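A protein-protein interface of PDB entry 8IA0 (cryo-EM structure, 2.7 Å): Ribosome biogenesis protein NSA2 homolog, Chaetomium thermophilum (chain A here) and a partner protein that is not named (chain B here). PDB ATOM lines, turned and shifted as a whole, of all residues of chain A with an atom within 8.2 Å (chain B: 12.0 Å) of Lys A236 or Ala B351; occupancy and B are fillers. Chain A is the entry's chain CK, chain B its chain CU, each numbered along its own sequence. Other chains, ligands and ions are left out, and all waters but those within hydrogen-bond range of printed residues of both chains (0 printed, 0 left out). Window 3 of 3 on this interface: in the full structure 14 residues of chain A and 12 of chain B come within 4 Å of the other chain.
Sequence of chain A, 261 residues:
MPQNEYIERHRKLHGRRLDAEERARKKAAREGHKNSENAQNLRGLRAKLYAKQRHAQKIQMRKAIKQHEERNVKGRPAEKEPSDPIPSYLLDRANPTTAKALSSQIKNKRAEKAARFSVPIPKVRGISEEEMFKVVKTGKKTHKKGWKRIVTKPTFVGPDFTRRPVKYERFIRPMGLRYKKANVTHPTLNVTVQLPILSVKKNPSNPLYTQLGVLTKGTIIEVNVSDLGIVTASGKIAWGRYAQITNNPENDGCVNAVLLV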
ATOM      1  N   GLU A 222       9.652  -1.367 -26.472  1.00  0.00           N
ATOM      2  CA  GLU A 222       8.536  -2.120 -25.918  1.00  0.00           C
ATOM      3  C   GLU A 222       9.106  -3.300 -25.147  1.00  0.00           C
ATOM      4  O   GLU A 222       9.884  -4.086 -25.698  1.00  0.00           O
ATOM      5  CB  GLU A 222       7.588  -2.577 -27.028  1.00  0.00           C
ATOM      6  CG  GLU A 222       6.231  -3.042 -26.546  1.00  0.00           C
ATOM      7  CD  GLU A 222       6.179  -4.535 -26.318  1.00  0.00           C
ATOM      8  OE1 GLU A 222       6.414  -5.292 -27.283  1.00  0.00           O
ATOM      9  OE2 GLU A 222       5.913  -4.951 -25.173  1.00  0.00           O
ATOM     10  N   VAL A 223       8.730  -3.419 -23.876  1.00  0.00           N
ATOM     11  CA  VAL A 223       9.355  -4.366 -22.962  1.00  0.00           C
ATOM     12  C   VAL A 223       8.297  -5.300 -22.395  1.00  0.00           C
ATOM     13  O   VAL A 223       7.104  -4.984 -22.371  1.00  0.00           O
ATOM     14  CB  VAL A 223      10.105  -3.644 -21.822  1.00  0.00           C
ATOM     15  CG1 VAL A 223      11.260  -2.834 -22.376  1.00  0.00           C
ATOM     16  CG2 VAL A 223       9.157  -2.755 -21.045  1.00  0.00           C
ATOM     17  N   ASN A 224       8.750  -6.464 -21.938  1.00  0.00           N
ATOM     18  CA  ASN A 224       7.876  -7.480 -21.368  1.00  0.00           C
ATOM     19  C   ASN A 224       7.770  -7.242 -19.866  1.00  0.00           C
ATOM     20  O   ASN A 224       8.747  -7.424 -19.133  1.00  0.00           O
ATOM     21  CB  ASN A 224       8.424  -8.876 -21.667  1.00  0.00           C
ATOM     22  CG  ASN A 224       7.540  -9.986 -21.132  1.00  0.00           C
ATOM     23  OD1 ASN A 224       6.468  -9.738 -20.582  1.00  0.00           O
ATOM     24  ND2 ASN A 224       7.992 -11.222 -21.293  1.00  0.00           N
ATOM     25  N   VAL A 225       6.584  -6.844 -19.412  1.00  0.00           N
ATOM     26  CA  VAL A 225       6.378  -6.449 -18.024  1.00  0.00           C
ATOM     27  C   VAL A 225       5.558  -7.504 -17.296  1.00  0.00           C
ATOM     28  O   VAL A 225       4.887  -7.204 -16.303  1.00  0.00           O
ATOM     29  CB  VAL A 225       5.691  -5.074 -17.941  1.00  0.00           C
ATOM     30  CG1 VAL A 225       6.683  -3.970 -18.253  1.00  0.00           C
ATOM     31  CG2 VAL A 225       4.514  -5.016 -18.893  1.00  0.00           C
ATOM     32  N   SER A 226       5.605  -8.744 -17.783  1.00  0.00           N
ATOM     33  CA  SER A 226       4.778  -9.796 -17.202  1.00  0.00           C
ATOM     34  C   SER A 226       5.194 -10.127 -15.775  1.00  0.00           C
ATOM     35  O   SER A 226       4.343 -10.484 -14.953  1.00  0.00           O
ATOM     36  CB  SER A 226       4.832 -11.048 -18.076  1.00  0.00           C
ATOM     37  OG  SER A 226       6.169 -11.431 -18.339  1.00  0.00           O
ATOM     38  N   GLY A 229       3.550  -7.740 -12.923  1.00  0.00           N
ATOM     39  CA  GLY A 229       2.171  -8.035 -12.587  1.00  0.00           C
ATOM     40  C   GLY A 229       1.313  -6.798 -12.434  1.00  0.00           C
ATOM     41  O   GLY A 229       0.712  -6.576 -11.379  1.00  0.00           O
ATOM     42  N   ILE A 230       1.248  -5.983 -13.481  1.00  0.00           N
ATOM     43  CA  ILE A 230       0.426  -4.779 -13.464  1.00  0.00           C
ATOM     44  C   ILE A 230      -0.997  -5.148 -13.856  1.00  0.00           C
ATOM     45  O   ILE A 230      -1.223  -5.810 -14.877  1.00  0.00           O
ATOM     46  CB  ILE A 230       1.004  -3.713 -14.407  1.00  0.00           C
ATOM     47  CG1 ILE A 230       2.528  -3.686 -14.311  1.00  0.00           C
ATOM     48  CG2 ILE A 230       0.427  -2.348 -14.082  1.00  0.00           C
ATOM     49  CD1 ILE A 230       3.181  -2.725 -15.274  1.00  0.00           C
ATOM     50  N   VAL A 231      -1.961  -4.723 -13.048  1.00  0.00           N
ATOM     51  CA  VAL A 231      -3.366  -5.034 -13.283  1.00  0.00           C
ATOM     52  C   VAL A 231      -4.000  -3.878 -14.045  1.00  0.00           C
ATOM     53  O   VAL A 231      -3.987  -2.735 -13.581  1.00  0.00           O
ATOM     54  CB  VAL A 231      -4.106  -5.297 -11.964  1.00  0.00           C
ATOM     55  CG1 VAL A 231      -5.606  -5.348 -12.198  1.00  0.00           C
ATOM     56  CG2 VAL A 231      -3.616  -6.589 -11.333  1.00  0.00           C
ATOM     57  N   THR A 232      -4.555  -4.178 -15.216  1.00  0.00           N
ATOM     58  CA  THR A 232      -5.204  -3.169 -16.034  1.00  0.00           C
ATOM     59  C   THR A 232      -6.618  -2.897 -15.527  1.00  0.00           C
ATOM     60  O   THR A 232      -7.124  -3.559 -14.617  1.00  0.00           O
ATOM     61  CB  THR A 232      -5.244  -3.607 -17.496  1.00  0.00           C
ATOM     62  OG1 THR A 232      -6.435  -4.368 -17.735  1.00  0.00           O
ATOM     63  CG2 THR A 232      -4.030  -4.458 -17.830  1.00  0.00           C
ATOM     64  N   ALA A 233      -7.259  -1.893 -16.131  1.00  0.00           N
ATOM     65  CA  ALA A 233      -8.620  -1.542 -15.741  1.00  0.00           C
ATOM     66  C   ALA A 233      -9.599  -2.672 -16.029  1.00  0.00           C
ATOM     67  O   ALA A 233     -10.640  -2.774 -15.371  1.00  0.00           O
ATOM     68  CB  ALA A 233      -9.059  -0.265 -16.456  1.00  0.00           C
ATOM     69  N   SER A 234      -9.287  -3.524 -17.005  1.00  0.00           N
ATOM     70  CA  SER A 234     -10.133  -4.665 -17.327  1.00  0.00           C
ATOM     71  C   SER A 234      -9.853  -5.877 -16.450  1.00  0.00           C
ATOM     72  O   SER A 234     -10.526  -6.901 -16.609  1.00  0.00           O
ATOM     73  CB  SER A 234      -9.961  -5.047 -18.798  1.00  0.00           C
ATOM     74  OG  SER A 234     -10.715  -6.205 -19.112  1.00  0.00           O
ATOM     75  N   GLY A 235      -8.884  -5.792 -15.541  1.00  0.00           N
ATOM     76  CA  GLY A 235      -8.556  -6.896 -14.667  1.00  0.00           C
ATOM     77  C   GLY A 235      -7.507  -7.848 -15.196  1.00  0.00           C
ATOM     78  O   GLY A 235      -7.176  -8.821 -14.508  1.00  0.00           O
ATOM     79  N   LYS A 236      -6.976  -7.603 -16.387  1.00  0.00           N
ATOM     80  CA  LYS A 236      -5.956  -8.460 -16.969  1.00  0.00           C
ATOM     81  C   LYS A 236      -4.569  -8.051 -16.483  1.00  0.00           C
ATOM     82  O   LYS A 236      -4.383  -7.003 -15.861  1.00  0.00           O
ATOM     83  CB  LYS A 236      -6.020  -8.403 -18.495  1.00  0.00           C
ATOM     84  CG  LYS A 236      -7.433  -8.481 -19.056  1.00  0.00           C
ATOM     85  CD  LYS A 236      -7.439  -8.947 -20.503  1.00  0.00           C
ATOM     86  CE  LYS A 236      -6.364  -8.248 -21.320  1.00  0.00           C
ATOM     87  NZ  LYS A 236      -6.617  -6.786 -21.438  1.00  0.00           N
ATOM     88  N   ILE A 237      -3.593  -8.903 -16.769  1.00  0.00           N
ATOM     89  CA  ILE A 237      -2.204  -8.653 -16.397  1.00  0.00           C
ATOM     90  C   ILE A 237      -1.462  -8.182 -17.641  1.00  0.00           C
ATOM     91  O   ILE A 237      -1.464  -8.863 -18.672  1.00  0.00           O
ATOM     92  CB  ILE A 237      -1.546  -9.906 -15.796  1.00  0.00           C
ATOM     93  CG1 ILE A 237      -1.843 -10.038 -14.295  1.00  0.00           C
ATOM     94  CG2 ILE A 237      -0.043  -9.884 -16.015  1.00  0.00           C
ATOM     95  CD1 ILE A 237      -3.308 -10.062 -13.913  1.00  0.00           C
ATOM     96  N   ALA A 238      -0.843  -7.009 -17.552  1.00  0.00           N
ATOM     97  CA  ALA A 238      -0.165  -6.424 -18.701  1.00  0.00           C
ATOM     98  C   ALA A 238       1.070  -7.234 -19.075  1.00  0.00           C
ATOM     99  O   ALA A 238       1.829  -7.680 -18.211  1.00  0.00           O
ATOM    100  CB  ALA A 238       0.228  -4.979 -18.403  1.00  0.00           C
ATOM    101  N   TRP A 239       1.270  -7.419 -20.378  1.00  0.00           N
ATOM    102  CA  TRP A 239       2.384  -8.201 -20.890  1.00  0.00           C
ATOM    103  C   TRP A 239       3.353  -7.388 -21.734  1.00  0.00           C
ATOM    104  O   TRP A 239       4.400  -7.913 -22.125  1.00  0.00           O
ATOM    105  CB  TRP A 239       1.865  -9.389 -21.705  1.00  0.00           C
ATOM    106  CG  TRP A 239       1.738 -10.636 -20.901  1.00  0.00           C
ATOM    107  CD1 TRP A 239       0.831 -10.886 -19.917  1.00  0.00           C
ATOM    108  CD2 TRP A 239       2.557 -11.803 -20.999  1.00  0.00           C
ATOM    109  NE1 TRP A 239       1.029 -12.140 -19.399  1.00  0.00           N
ATOM    110  CE2 TRP A 239       2.084 -12.724 -20.047  1.00  0.00           C
ATOM    111  CE3 TRP A 239       3.643 -12.160 -21.800  1.00  0.00           C
ATOM    112  CZ2 TRP A 239       2.658 -13.979 -19.874  1.00  0.00           C
ATOM    113  CZ3 TRP A 239       4.210 -13.405 -21.629  1.00  0.00           C
ATOM    114  CH2 TRP A 239       3.718 -14.300 -20.675  1.00  0.00           C
ATOM    115  N   GLY A 240       3.039  -6.130 -22.026  1.00  0.00           N
ATOM    116  CA  GLY A 240       3.935  -5.309 -22.813  1.00  0.00           C
ATOM    117  C   GLY A 240       3.622  -3.831 -22.735  1.00  0.00           C
ATOM    118  O   GLY A 240       2.474  -3.423 -22.934  1.00  0.00           O
ATOM    119  N   ARG A 241       4.636  -3.016 -22.452  1.00  0.00           N
ATOM    120  CA  ARG A 241       4.450  -1.584 -22.284  1.00  0.00           C
ATOM    121  C   ARG A 241       5.646  -0.842 -22.863  1.00  0.00           C
ATOM    122  O   ARG A 241       6.741  -1.392 -22.995  1.00  0.00           O
ATOM    123  CB  ARG A 241       4.259  -1.210 -20.811  1.00  0.00           C
ATOM    124  CG  ARG A 241       2.962  -1.709 -20.207  1.00  0.00           C
ATOM    125  CD  ARG A 241       1.801  -0.820 -20.597  1.00  0.00           C
ATOM    126  NE  ARG A 241       0.617  -1.076 -19.788  1.00  0.00           N
ATOM    127  CZ  ARG A 241      -0.317  -1.968 -20.085  1.00  0.00           C
ATOM    128  NH1 ARG A 241      -0.238  -2.715 -21.173  1.00  0.00           N
ATOM    129  NH2 ARG A 241      -1.358  -2.114 -19.270  1.00  0.00           N
ATOM    130  N   ARG B 341      -0.147   9.494 -19.224  1.00  0.00           N
ATOM    131  CA  ARG B 341      -0.177   8.215 -18.523  1.00  0.00           C
ATOM    132  C   ARG B 341      -0.046   8.411 -17.018  1.00  0.00           C
ATOM    133  O   ARG B 341      -0.732   7.742 -16.237  1.00  0.00           O
ATOM    134  CB  ARG B 341       0.932   7.300 -19.043  1.00  0.00           C
ATOM    135  CG  ARG B 341       0.836   6.973 -20.522  1.00  0.00           C
ATOM    136  CD  ARG B 341       0.150   5.643 -20.761  1.00  0.00           C
ATOM    137  NE  ARG B 341       0.266   5.217 -22.150  1.00  0.00           N
ATOM    138  CZ  ARG B 341       0.991   4.187 -22.563  1.00  0.00           C
ATOM    139  NH1 ARG B 341       1.678   3.441 -21.714  1.00  0.00           N
ATOM    140  NH2 ARG B 341       1.027   3.895 -23.859  1.00  0.00           N
ATOM    141  N   GLY B 345      -4.478   6.756 -16.921  1.00  0.00           N
ATOM    142  CA  GLY B 345      -4.476   5.898 -18.091  1.00  0.00           C
ATOM    143  C   GLY B 345      -3.185   5.123 -18.271  1.00  0.00           C
ATOM    144  O   GLY B 345      -3.088   3.963 -17.871  1.00  0.00           O
ATOM    145  N   ALA B 348      -6.156   2.187 -18.404  1.00  0.00           N
ATOM    146  CA  ALA B 348      -7.033   2.396 -19.549  1.00  0.00           C
ATOM    147  C   ALA B 348      -6.497   1.692 -20.792  1.00  0.00           C
ATOM    148  O   ALA B 348      -7.050   1.832 -21.881  1.00  0.00           O
ATOM    149  CB  ALA B 348      -7.207   3.881 -19.816  1.00  0.00           C
ATOM    150  N   LEU B 349      -5.417   0.934 -20.620  1.00  0.00           N
ATOM    151  CA  LEU B 349      -4.768   0.233 -21.715  1.00  0.00           C
ATOM    152  C   LEU B 349      -5.129  -1.250 -21.681  1.00  0.00           C
ATOM    153  O   LEU B 349      -5.802  -1.737 -20.771  1.00  0.00           O
ATOM    154  CB  LEU B 349      -3.251   0.423 -21.648  1.00  0.00           C
ATOM    155  CG  LEU B 349      -2.674   1.686 -22.286  1.00  0.00           C
ATOM    156  CD1 LEU B 349      -2.808   2.876 -21.350  1.00  0.00           C
ATOM    157  CD2 LEU B 349      -1.223   1.466 -22.674  1.00  0.00           C
ATOM    158  N   GLY B 350      -4.669  -1.974 -22.696  1.00  0.00           N
ATOM    159  CA  GLY B 350      -4.870  -3.400 -22.797  1.00  0.00           C
ATOM    160  C   GLY B 350      -3.701  -4.189 -22.248  1.00  0.00           C
ATOM    161  O   GLY B 350      -2.909  -3.699 -21.434  1.00  0.00           O
ATOM    162  N   ALA B 351      -3.592  -5.438 -22.700  1.00  0.00           N
ATOM    163  CA  ALA B 351      -2.494  -6.290 -22.260  1.00  0.00           C
ATOM    164  C   ALA B 351      -1.198  -5.937 -22.978  1.00  0.00           C
ATOM    165  O   ALA B 351      -0.149  -5.779 -22.344  1.00  0.00           O
ATOM    166  CB  ALA B 351      -2.846  -7.760 -22.481  1.00  0.00           C
ATOM    167  N   THR B 352      -1.253  -5.808 -24.298  1.00  0.00           N
ATOM    168  CA  THR B 352      -0.108  -5.436 -25.111  1.00  0.00           C
ATOM    169  C   THR B 352      -0.365  -4.078 -25.749  1.00  0.00           C
ATOM    170  O   THR B 352      -1.512  -3.641 -25.875  1.00  0.00           O
ATOM    171  CB  THR B 352       0.165  -6.486 -26.193  1.00  0.00           C
ATOM    172  OG1 THR B 352      -0.065  -7.794 -25.654  1.00  0.00           O
ATOM    173  CG2 THR B 352       1.605  -6.405 -26.673  1.00  0.00           C
ATOM    174  N   GLU B 353       0.712  -3.406 -26.142  1.00  0.00           N
ATOM    175  CA  GLU B 353       0.581  -2.090 -26.745  1.00  0.00           C
ATOM    176  C   GLU B 353      -0.029  -2.196 -28.139  1.00  0.00           C
ATOM    177  O   GLU B 353      -0.102  -3.273 -28.739  1.00  0.00           O
ATOM    178  CB  GLU B 353       1.936  -1.388 -26.807  1.00  0.00           C
ATOM    179  CG  GLU B 353       2.563  -1.168 -25.444  1.00  0.00           C
ATOM    180  CD  GLU B 353       2.151   0.148 -24.816  1.00  0.00           C
ATOM    181  OE1 GLU B 353       1.064   0.660 -25.157  1.00  0.00           O
ATOM    182  OE2 GLU B 353       2.908   0.670 -23.971  1.00  0.00           O
ATOM    183  N   ALA B 354      -0.479  -1.053 -28.649  1.00  0.00           N
ATOM    184  CA  ALA B 354      -1.194  -1.024 -29.916  1.00  0.00           C
ATOM    185  C   ALA B 354      -0.296  -1.482 -31.059  1.00  0.00           C
ATOM    186  O   ALA B 354       0.900  -1.184 -31.092  1.00  0.00           O
ATOM    187  CB  ALA B 354      -1.726   0.383 -30.183  1.00  0.00           C
ATOM    188  N   ASP B 355      -0.889  -2.216 -32.004  1.00  0.00           N
ATOM    189  CA  ASP B 355      -0.109  -2.822 -33.079  1.00  0.00           C
ATOM    190  C   ASP B 355       0.288  -1.808 -34.145  1.00  0.00           C
ATOM    191  O   ASP B 355       1.260  -2.034 -34.875  1.00  0.00           O
ATOM    192  CB  ASP B 355      -0.895  -3.968 -33.710  1.00  0.00           C
ATOM    193  CG  ASP B 355       0.003  -5.054 -34.267  1.00  0.00           C
ATOM    194  OD1 ASP B 355       1.163  -5.156 -33.815  1.00  0.00           O
ATOM    195  OD2 ASP B 355      -0.450  -5.805 -35.155  1.00  0.00           O
ATOM    196  N   GLU B 365      -4.089   8.014 -28.898  1.00  0.00           N
ATOM    197  CA  GLU B 365      -4.191   8.011 -27.442  1.00  0.00           C
ATOM    198  C   GLU B 365      -4.295   9.428 -26.890  1.00  0.00           C
ATOM    199  O   GLU B 365      -5.078   9.683 -25.968  1.00  0.00           O
ATOM    200  CB  GLU B 365      -2.999   7.272 -26.836  1.00  0.00           C
ATOM    201  CG  GLU B 365      -2.748   7.589 -25.373  1.00  0.00           C
ATOM    202  CD  GLU B 365      -2.315   6.372 -24.582  1.00  0.00           C
ATOM    203  OE1 GLU B 365      -1.099   6.099 -24.518  1.00  0.00           O
ATOM    204  OE2 GLU B 365      -3.194   5.684 -24.022  1.00  0.00           O
ATOM    205  N   ARG B 368      -7.999  10.539 -27.703  1.00  0.00           N
ATOM    206  CA  ARG B 368      -9.053   9.939 -26.894  1.00  0.00           C
ATOM    207  C   ARG B 368      -9.020  10.420 -25.449  1.00  0.00           C
ATOM    208  O   ARG B 368     -10.043  10.338 -24.761  1.00  0.00           O
ATOM    209  CB  ARG B 368      -8.952   8.412 -26.946  1.00  0.00           C
ATOM    210  CG  ARG B 368      -8.388   7.766 -25.692  1.00  0.00           C
ATOM    211  CD  ARG B 368      -8.008   6.315 -25.939  1.00  0.00           C
ATOM    212  NE  ARG B 368      -7.246   6.150 -27.171  1.00  0.00           N
ATOM    213  CZ  ARG B 368      -7.123   5.004 -27.826  1.00  0.00           C
ATOM    214  NH1 ARG B 368      -7.699   3.895 -27.394  1.00  0.00           N
ATOM    215  NH2 ARG B 368      -6.401   4.970 -28.943  1.00  0.00           N
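O of Ile A230 lies within hydrogen-bond range of N of Ala A238 (3.0 Å). The backbone NH (N) of Val A223 sits at hydrogen-bond distance from the backbone carbonyl oxygen (O) of Arg A241 (3.0 Å). The side-chain hydroxyl (OG1) of Thr A232 is in hydrogen-bond range of the backbone NH (N) of Ser A234, 3.1 Å away. OD1 of Asn A224 lies close to O of Trp A239 (3.2 Å). OE1 of Glu B353 lies within salt-bridge range of NH2 of Arg B341 (3.5 Å).
Printed residues of chain B within 4 Å of Lys A236: Gly B350 (3.99 Å) and Ala B351 (3.5 Å). Of chain A, only Lys A236 (3.5 Å), Ala A238 (3.7 Å), Trp A239 (2.9 Å), Gly A240 (3.2 Å) and Arg A241 (3.3 Å) come within 4 Å of Ala B351. No residue of chain B comes within 4 Å of Val A231. No residue of chain B comes within 4 Å of Ser A234. No residue of chain B comes within 4 Å of Gly A235. Gly A240 touches just these residues of chain B: Ala B351 (3.2 Å), Thr B352 (3.9 Å) and Glu B353 (3.4 Å). Of the printed residues of chain A, Thr B352 touches Gly A240 (3.9 Å). Of the printed residues of chain A, Gly B350 touches Thr A232, Lys A236 and Arg A241. Of the printed residues of chain B, Trp A239 touches Ala B351.
Of the 18 printed residues of chain A, 6 touch a printed residue of chain B. Of the 12 printed residues of chain B, 5 touch a printed residue of chain A. Hydrophobic or aromatic side chains of chain B within 4 Å of the printed part of chain A: Leu B349 and Ala B351. Among the printed residues, 13 pairs touch across the chains. Among the printed residues, no Asp or Glu carboxylate lies within 4 Å of a Lys or Arg side-chain nitrogen of the other chain.
Among the printed residues, merely in contact across the chains: Thr A232 with Leu B349 (3.8 Å), Thr A232 with Gly B350 (3.8 Å), Lys A236 with Gly B350 (3.99 Å), Lys A236 with Ala B351 (3.5 Å), Ala A238 with Ala B351 (3.7 Å), Gly A240 with Thr B352 (3.9 Å), Gly A240 with Glu B353 (3.4 Å), Arg A241 with Leu B349 (3.96 Å) and Arg A241 with Glu B353 (3.2 Å).
The backbone carbonyl oxygen of Ala B351 sits at hydrogen-bond distance from the guanidinium group of Arg A241, 3.3 Å away. The guanidinium group (NH1) of Arg A241 is in hydrogen-bond range of the backbone carbonyl oxygen (O) of Gly B350, at 2.9 Å. The backbone carbonyl oxygen (O) of Ala B351 sits at hydrogen-bond distance from the backbone NH (N) of Trp A239 (2.9 Å). The backbone carbonyl oxygen (O) of Ala B351 is in hydrogen-bond range of the backbone NH (N) of Gly A240.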
